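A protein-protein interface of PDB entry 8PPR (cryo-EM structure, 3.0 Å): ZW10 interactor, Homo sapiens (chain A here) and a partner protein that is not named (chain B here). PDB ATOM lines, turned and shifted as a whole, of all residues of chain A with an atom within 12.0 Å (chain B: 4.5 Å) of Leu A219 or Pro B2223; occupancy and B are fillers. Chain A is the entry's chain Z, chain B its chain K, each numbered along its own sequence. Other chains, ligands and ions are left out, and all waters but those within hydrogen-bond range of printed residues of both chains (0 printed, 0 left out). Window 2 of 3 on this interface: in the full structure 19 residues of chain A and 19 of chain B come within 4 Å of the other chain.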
ATOM      1  N   GLN A 210      11.424  35.783 -17.064  1.00  0.00           N
ATOM      2  CA  GLN A 210      10.812  35.743 -18.389  1.00  0.00           C
ATOM      3  C   GLN A 210      11.434  34.648 -19.255  1.00  0.00           C
ATOM      4  O   GLN A 210      10.722  33.792 -19.806  1.00  0.00           O
ATOM      5  CB  GLN A 210      10.929  37.107 -19.066  1.00  0.00           C
ATOM      6  CG  GLN A 210      10.008  38.153 -18.466  1.00  0.00           C
ATOM      7  CD  GLN A 210      10.041  39.465 -19.220  1.00  0.00           C
ATOM      8  OE1 GLN A 210      11.075  40.127 -19.295  1.00  0.00           O
ATOM      9  NE2 GLN A 210       8.905  39.843 -19.792  1.00  0.00           N
ATOM     10  N   THR A 211      12.766  34.636 -19.364  1.00  0.00           N
ATOM     11  CA  THR A 211      13.411  33.603 -20.168  1.00  0.00           C
ATOM     12  C   THR A 211      13.289  32.241 -19.499  1.00  0.00           C
ATOM     13  O   THR A 211      13.168  31.221 -20.182  1.00  0.00           O
ATOM     14  CB  THR A 211      14.876  33.963 -20.442  1.00  0.00           C
ATOM     15  OG1 THR A 211      15.413  33.062 -21.419  1.00  0.00           O
ATOM     16  CG2 THR A 211      15.722  33.873 -19.175  1.00  0.00           C
ATOM     17  N   PHE A 212      13.293  32.209 -18.165  1.00  0.00           N
ATOM     18  CA  PHE A 212      13.025  30.977 -17.433  1.00  0.00           C
ATOM     19  C   PHE A 212      11.693  30.365 -17.864  1.00  0.00           C
ATOM     20  O   PHE A 212      11.631  29.208 -18.299  1.00  0.00           O
ATOM     21  CB  PHE A 212      13.036  31.314 -15.938  1.00  0.00           C
ATOM     22  CG  PHE A 212      12.812  30.152 -15.030  1.00  0.00           C
ATOM     23  CD1 PHE A 212      13.805  29.229 -14.783  1.00  0.00           C
ATOM     24  CD2 PHE A 212      11.606  30.006 -14.376  1.00  0.00           C
ATOM     25  CE1 PHE A 212      13.589  28.165 -13.929  1.00  0.00           C
ATOM     26  CE2 PHE A 212      11.392  28.955 -13.530  1.00  0.00           C
ATOM     27  CZ  PHE A 212      12.377  28.034 -13.302  1.00  0.00           C
ATOM     28  N   LEU A 213      10.627  31.165 -17.812  1.00  0.00           N
ATOM     29  CA  LEU A 213       9.296  30.677 -18.145  1.00  0.00           C
ATOM     30  C   LEU A 213       9.204  30.261 -19.603  1.00  0.00           C
ATOM     31  O   LEU A 213       8.567  29.252 -19.923  1.00  0.00           O
ATOM     32  CB  LEU A 213       8.258  31.749 -17.826  1.00  0.00           C
ATOM     33  CG  LEU A 213       6.792  31.358 -18.024  1.00  0.00           C
ATOM     34  CD1 LEU A 213       6.427  30.190 -17.122  1.00  0.00           C
ATOM     35  CD2 LEU A 213       5.882  32.546 -17.763  1.00  0.00           C
ATOM     36  N   GLN A 214       9.820  31.021 -20.510  1.00  0.00           N
ATOM     37  CA  GLN A 214       9.673  30.640 -21.910  1.00  0.00           C
ATOM     38  C   GLN A 214      10.541  29.436 -22.282  1.00  0.00           C
ATOM     39  O   GLN A 214      10.170  28.677 -23.186  1.00  0.00           O
ATOM     40  CB  GLN A 214       9.908  31.848 -22.827  1.00  0.00           C
ATOM     41  CG  GLN A 214      11.248  32.561 -22.782  1.00  0.00           C
ATOM     42  CD  GLN A 214      12.264  32.007 -23.758  1.00  0.00           C
ATOM     43  OE1 GLN A 214      11.906  31.406 -24.772  1.00  0.00           O
ATOM     44  NE2 GLN A 214      13.532  32.298 -23.512  1.00  0.00           N
ATOM     45  N   LEU A 215      11.659  29.196 -21.586  1.00  0.00           N
ATOM     46  CA  LEU A 215      12.312  27.895 -21.730  1.00  0.00           C
ATOM     47  C   LEU A 215      11.441  26.761 -21.210  1.00  0.00           C
ATOM     48  O   LEU A 215      11.389  25.695 -21.828  1.00  0.00           O
ATOM     49  CB  LEU A 215      13.689  27.853 -21.065  1.00  0.00           C
ATOM     50  CG  LEU A 215      14.904  28.369 -21.843  1.00  0.00           C
ATOM     51  CD1 LEU A 215      15.103  27.479 -23.064  1.00  0.00           C
ATOM     52  CD2 LEU A 215      14.814  29.800 -22.266  1.00  0.00           C
ATOM     53  N   LEU A 216      10.769  26.943 -20.072  1.00  0.00           N
ATOM     54  CA  LEU A 216       9.846  25.883 -19.660  1.00  0.00           C
ATOM     55  C   LEU A 216       8.735  25.678 -20.688  1.00  0.00           C
ATOM     56  O   LEU A 216       8.299  24.543 -20.915  1.00  0.00           O
ATOM     57  CB  LEU A 216       9.270  26.139 -18.266  1.00  0.00           C
ATOM     58  CG  LEU A 216      10.127  25.826 -17.027  1.00  0.00           C
ATOM     59  CD1 LEU A 216      11.291  26.758 -16.770  1.00  0.00           C
ATOM     60  CD2 LEU A 216       9.225  25.762 -15.807  1.00  0.00           C
ATOM     61  N   TYR A 217       8.279  26.753 -21.335  1.00  0.00           N
ATOM     62  CA  TYR A 217       7.316  26.597 -22.424  1.00  0.00           C
ATOM     63  C   TYR A 217       7.891  25.776 -23.572  1.00  0.00           C
ATOM     64  O   TYR A 217       7.229  24.864 -24.083  1.00  0.00           O
ATOM     65  CB  TYR A 217       6.859  27.961 -22.939  1.00  0.00           C
ATOM     66  CG  TYR A 217       6.007  28.757 -21.980  1.00  0.00           C
ATOM     67  CD1 TYR A 217       5.431  28.159 -20.869  1.00  0.00           C
ATOM     68  CD2 TYR A 217       5.755  30.102 -22.205  1.00  0.00           C
ATOM     69  CE1 TYR A 217       4.639  28.881 -19.998  1.00  0.00           C
ATOM     70  CE2 TYR A 217       4.966  30.834 -21.340  1.00  0.00           C
ATOM     71  CZ  TYR A 217       4.412  30.219 -20.244  1.00  0.00           C
ATOM     72  OH  TYR A 217       3.622  30.940 -19.373  1.00  0.00           O
ATOM     73  N   THR A 218       9.116  26.087 -23.999  1.00  0.00           N
ATOM     74  CA  THR A 218       9.697  25.377 -25.137  1.00  0.00           C
ATOM     75  C   THR A 218       9.969  23.914 -24.803  1.00  0.00           C
ATOM     76  O   THR A 218       9.751  23.029 -25.638  1.00  0.00           O
ATOM     77  CB  THR A 218      10.980  26.070 -25.598  1.00  0.00           C
ATOM     78  OG1 THR A 218      11.801  26.372 -24.462  1.00  0.00           O
ATOM     79  CG2 THR A 218      10.651  27.360 -26.335  1.00  0.00           C
ATOM     80  N   LEU A 219      10.450  23.642 -23.588  1.00  0.00           N
ATOM     81  CA  LEU A 219      10.723  22.266 -23.184  1.00  0.00           C
ATOM     82  C   LEU A 219       9.439  21.465 -23.012  1.00  0.00           C
ATOM     83  O   LEU A 219       9.393  20.279 -23.356  1.00  0.00           O
ATOM     84  CB  LEU A 219      11.546  22.248 -21.892  1.00  0.00           C
ATOM     85  CG  LEU A 219      13.070  22.408 -21.962  1.00  0.00           C
ATOM     86  CD1 LEU A 219      13.664  21.235 -22.709  1.00  0.00           C
ATOM     87  CD2 LEU A 219      13.521  23.708 -22.607  1.00  0.00           C
ATOM     88  N   GLN A 220       8.385  22.089 -22.481  1.00  0.00           N
ATOM     89  CA  GLN A 220       7.130  21.377 -22.286  1.00  0.00           C
ATOM     90  C   GLN A 220       6.390  21.118 -23.591  1.00  0.00           C
ATOM     91  O   GLN A 220       5.475  20.286 -23.609  1.00  0.00           O
ATOM     92  CB  GLN A 220       6.230  22.155 -21.326  1.00  0.00           C
ATOM     93  CG  GLN A 220       5.304  21.276 -20.505  1.00  0.00           C
ATOM     94  CD  GLN A 220       5.961  20.772 -19.236  1.00  0.00           C
ATOM     95  OE1 GLN A 220       6.838  21.430 -18.675  1.00  0.00           O
ATOM     96  NE2 GLN A 220       5.541  19.600 -18.776  1.00  0.00           N
ATOM     97  N   GLY A 221       6.758  21.797 -24.671  1.00  0.00           N
ATOM     98  CA  GLY A 221       6.115  21.602 -25.956  1.00  0.00           C
ATOM     99  C   GLY A 221       7.008  21.989 -27.118  1.00  0.00           C
ATOM    100  O   GLY A 221       7.140  21.242 -28.087  1.00  0.00           O
ATOM    101  N   TRP B2135      10.395  15.712 -15.430  1.00  0.00           N
ATOM    102  CA  TRP B2135      11.815  16.020 -15.399  1.00  0.00           C
ATOM    103  C   TRP B2135      12.072  17.330 -14.668  1.00  0.00           C
ATOM    104  O   TRP B2135      11.199  18.197 -14.573  1.00  0.00           O
ATOM    105  CB  TRP B2135      12.382  16.091 -16.818  1.00  0.00           C
ATOM    106  CG  TRP B2135      11.431  16.693 -17.807  1.00  0.00           C
ATOM    107  CD1 TRP B2135      10.649  16.021 -18.699  1.00  0.00           C
ATOM    108  CD2 TRP B2135      11.150  18.085 -18.000  1.00  0.00           C
ATOM    109  NE1 TRP B2135       9.904  16.904 -19.439  1.00  0.00           N
ATOM    110  CE2 TRP B2135      10.193  18.179 -19.029  1.00  0.00           C
ATOM    111  CE3 TRP B2135      11.618  19.260 -17.405  1.00  0.00           C
ATOM    112  CZ2 TRP B2135       9.694  19.401 -19.475  1.00  0.00           C
ATOM    113  CZ3 TRP B2135      11.120  20.472 -17.849  1.00  0.00           C
ATOM    114  CH2 TRP B2135      10.168  20.533 -18.874  1.00  0.00           C
ATOM    115  N   PHE B2147      19.470  17.708 -16.986  1.00  0.00           N
ATOM    116  CA  PHE B2147      18.182  17.274 -16.471  1.00  0.00           C
ATOM    117  C   PHE B2147      18.385  16.173 -15.442  1.00  0.00           C
ATOM    118  O   PHE B2147      19.245  15.303 -15.598  1.00  0.00           O
ATOM    119  CB  PHE B2147      17.276  16.763 -17.593  1.00  0.00           C
ATOM    120  CG  PHE B2147      16.938  17.798 -18.621  1.00  0.00           C
ATOM    121  CD1 PHE B2147      17.826  18.098 -19.640  1.00  0.00           C
ATOM    122  CD2 PHE B2147      15.724  18.460 -18.580  1.00  0.00           C
ATOM    123  CE1 PHE B2147      17.514  19.050 -20.589  1.00  0.00           C
ATOM    124  CE2 PHE B2147      15.406  19.407 -19.531  1.00  0.00           C
ATOM    125  CZ  PHE B2147      16.302  19.706 -20.534  1.00  0.00           C
ATOM    126  N   GLN B2219      17.529  21.337 -31.650  1.00  0.00           N
ATOM    127  CA  GLN B2219      16.743  21.580 -30.446  1.00  0.00           C
ATOM    128  C   GLN B2219      15.255  21.317 -30.681  1.00  0.00           C
ATOM    129  O   GLN B2219      14.491  21.186 -29.718  1.00  0.00           O
ATOM    130  CB  GLN B2219      17.006  23.008 -29.955  1.00  0.00           C
ATOM    131  CG  GLN B2219      16.242  23.436 -28.713  1.00  0.00           C
ATOM    132  CD  GLN B2219      16.787  24.716 -28.110  1.00  0.00           C
ATOM    133  OE1 GLN B2219      17.956  25.056 -28.300  1.00  0.00           O
ATOM    134  NE2 GLN B2219      15.942  25.434 -27.380  1.00  0.00           N
ATOM    135  N   HIS B2220      14.824  21.225 -31.946  1.00  0.00           N
ATOM    136  CA  HIS B2220      13.426  20.914 -32.236  1.00  0.00           C
ATOM    137  C   HIS B2220      13.012  19.562 -31.671  1.00  0.00           C
ATOM    138  O   HIS B2220      11.942  19.433 -31.065  1.00  0.00           O
ATOM    139  CB  HIS B2220      13.177  20.935 -33.745  1.00  0.00           C
ATOM    140  CG  HIS B2220      13.275  22.293 -34.361  1.00  0.00           C
ATOM    141  ND1 HIS B2220      13.266  22.494 -35.724  1.00  0.00           N
ATOM    142  CD2 HIS B2220      13.342  23.523 -33.801  1.00  0.00           C
ATOM    143  CE1 HIS B2220      13.350  23.786 -35.980  1.00  0.00           C
ATOM    144  NE2 HIS B2220      13.398  24.433 -34.829  1.00  0.00           N
ATOM    145  N   GLN B2221      13.841  18.542 -31.864  1.00  0.00           N
ATOM    146  CA  GLN B2221      13.484  17.179 -31.503  1.00  0.00           C
ATOM    147  C   GLN B2221      13.819  16.850 -30.059  1.00  0.00           C
ATOM    148  O   GLN B2221      13.493  15.753 -29.593  1.00  0.00           O
ATOM    149  CB  GLN B2221      14.195  16.198 -32.433  1.00  0.00           C
ATOM    150  CG  GLN B2221      13.775  16.340 -33.880  1.00  0.00           C
ATOM    151  CD  GLN B2221      14.510  15.387 -34.791  1.00  0.00           C
ATOM    152  OE1 GLN B2221      15.369  14.629 -34.348  1.00  0.00           O
ATOM    153  NE2 GLN B2221      14.187  15.431 -36.079  1.00  0.00           N
ATOM    154  N   LEU B2222      14.468  17.769 -29.351  1.00  0.00           N
ATOM    155  CA  LEU B2222      14.773  17.536 -27.943  1.00  0.00           C
ATOM    156  C   LEU B2222      13.519  17.381 -27.093  1.00  0.00           C
ATOM    157  O   LEU B2222      13.460  16.429 -26.299  1.00  0.00           O
ATOM    158  CB  LEU B2222      15.686  18.657 -27.431  1.00  0.00           C
ATOM    159  CG  LEU B2222      16.285  18.535 -26.028  1.00  0.00           C
ATOM    160  CD1 LEU B2222      17.586  19.306 -25.951  1.00  0.00           C
ATOM    161  CD2 LEU B2222      15.329  19.045 -24.968  1.00  0.00           C
ATOM    162  N   PRO B2223      12.509  18.261 -27.173  1.00  0.00           N
ATOM    163  CA  PRO B2223      11.311  18.047 -26.339  1.00  0.00           C
ATOM    164  C   PRO B2223      10.572  16.756 -26.650  1.00  0.00           C
ATOM    165  O   PRO B2223      10.042  16.109 -25.736  1.00  0.00           O
ATOM    166  CB  PRO B2223      10.457  19.288 -26.638  1.00  0.00           C
ATOM    167  CG  PRO B2223      11.427  20.308 -27.121  1.00  0.00           C
ATOM    168  CD  PRO B2223      12.430  19.535 -27.906  1.00  0.00           C
ATOM    169  N   LYS B2224      10.499  16.369 -27.925  1.00  0.00           N
ATOM    170  CA  LYS B2224       9.826  15.123 -28.279  1.00  0.00           C
ATOM    171  C   LYS B2224      10.542  13.929 -27.664  1.00  0.00           C
ATOM    172  O   LYS B2224       9.911  13.032 -27.091  1.00  0.00           O
ATOM    173  CB  LYS B2224       9.746  14.984 -29.799  1.00  0.00           C
ATOM    174  CG  LYS B2224       9.339  13.597 -30.270  1.00  0.00           C
ATOM    175  CD  LYS B2224       7.976  13.209 -29.715  1.00  0.00           C
ATOM    176  CE  LYS B2224       7.482  11.905 -30.316  1.00  0.00           C
ATOM    177  NZ  LYS B2224       6.133  11.543 -29.802  1.00  0.00           N
ATOM    178  N   MET B2225      11.869  13.905 -27.777  1.00  0.00           N
ATOM    179  CA  MET B2225      12.656  12.858 -27.139  1.00  0.00           C
ATOM    180  C   MET B2225      12.478  12.896 -25.629  1.00  0.00           C
ATOM    181  O   MET B2225      12.448  11.854 -24.965  1.00  0.00           O
ATOM    182  CB  MET B2225      14.126  13.016 -27.531  1.00  0.00           C
ATOM    183  CG  MET B2225      15.069  11.951 -26.989  1.00  0.00           C
ATOM    184  SD  MET B2225      15.606  12.238 -25.292  1.00  0.00           S
ATOM    185  CE  MET B2225      16.720  13.619 -25.531  1.00  0.00           C
ATOM    186  N   LEU B2226      12.374  14.100 -25.067  1.00  0.00           N
ATOM    187  CA  LEU B2226      12.164  14.237 -23.631  1.00  0.00           C
ATOM    188  C   LEU B2226      10.860  13.582 -23.210  1.00  0.00           C
ATOM    189  O   LEU B2226      10.812  12.859 -22.214  1.00  0.00           O
ATOM    190  CB  LEU B2226      12.168  15.714 -23.240  1.00  0.00           C
ATOM    191  CG  LEU B2226      13.526  16.329 -22.918  1.00  0.00           C
ATOM    192  CD1 LEU B2226      13.341  17.662 -22.220  1.00  0.00           C
ATOM    193  CD2 LEU B2226      14.343  15.380 -22.060  1.00  0.00           C
ATOM    194  N   GLU B2227       9.790  13.830 -23.964  1.00  0.00           N
ATOM    195  CA  GLU B2227       8.512  13.182 -23.680  1.00  0.00           C
ATOM    196  C   GLU B2227       8.623  11.671 -23.831  1.00  0.00           C
ATOM    197  O   GLU B2227       8.122  10.907 -22.993  1.00  0.00           O
ATOM    198  CB  GLU B2227       7.432  13.739 -24.606  1.00  0.00           C
ATOM    199  CG  GLU B2227       6.022  13.270 -24.285  1.00  0.00           C
ATOM    200  CD  GLU B2227       5.701  11.924 -24.910  1.00  0.00           C
ATOM    201  OE1 GLU B2227       6.306  11.594 -25.952  1.00  0.00           O
ATOM    202  OE2 GLU B2227       4.850  11.196 -24.358  1.00  0.00           O
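O of Gln A214 lies within hydrogen-bond range of OG1 of Thr A218 (3.1 Å).
The side-chain hydroxyl of Thr A218 sits at hydrogen-bond distance from the backbone carbonyl oxygen of Leu A215.
Among the printed residues, merely in contact across the chains: Gln A220 with Trp B2135, Thr A218 with Pro B2223, Leu A219 with Leu B2222, Leu A219 with Pro B2223, Leu A219 with Leu B2226, Leu A219 with Trp B2135 and Leu A219 with Phe B2147.
Of chain A, only Thr A218 (3.5 Å) and Leu A219 (3.6 Å) come within 4 Å of Pro B2223.
No residue of chain A comes within 4 Å of Gln B2219.
Of the printed residues of chain A, Leu B2222 touches Leu A219 (3.6 Å).
No residue of chain A comes within 4 Å of Lys B2224.
No residue of chain A comes within 4 Å of Met B2225.
Of the printed residues of chain A, Leu B2226 touches Leu A219 (3.6 Å).
Of the printed residues of chain B, Thr A218 touches Pro B2223.
Of the printed residues of chain A, Phe B2147 touches Leu A219 (3.7 Å).
Of the printed residues of chain A, Trp B2135 touches Leu A219 and Gln A220.
Printed residues of chain B within 4 Å of Gln A220: Trp B2135 (3.5 Å).
Of the 11 printed residues of chain B, 5 touch a printed residue of chain A.
Hydrophobic or aromatic side chains of chain B that line the printed part of chain A: Trp B2135, Phe B2147, Leu B2222, Pro B2223 and Leu B2226.
Printed residues of chain A that touch a printed residue of chain B: Thr A218, Leu A219 and Gln A220.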
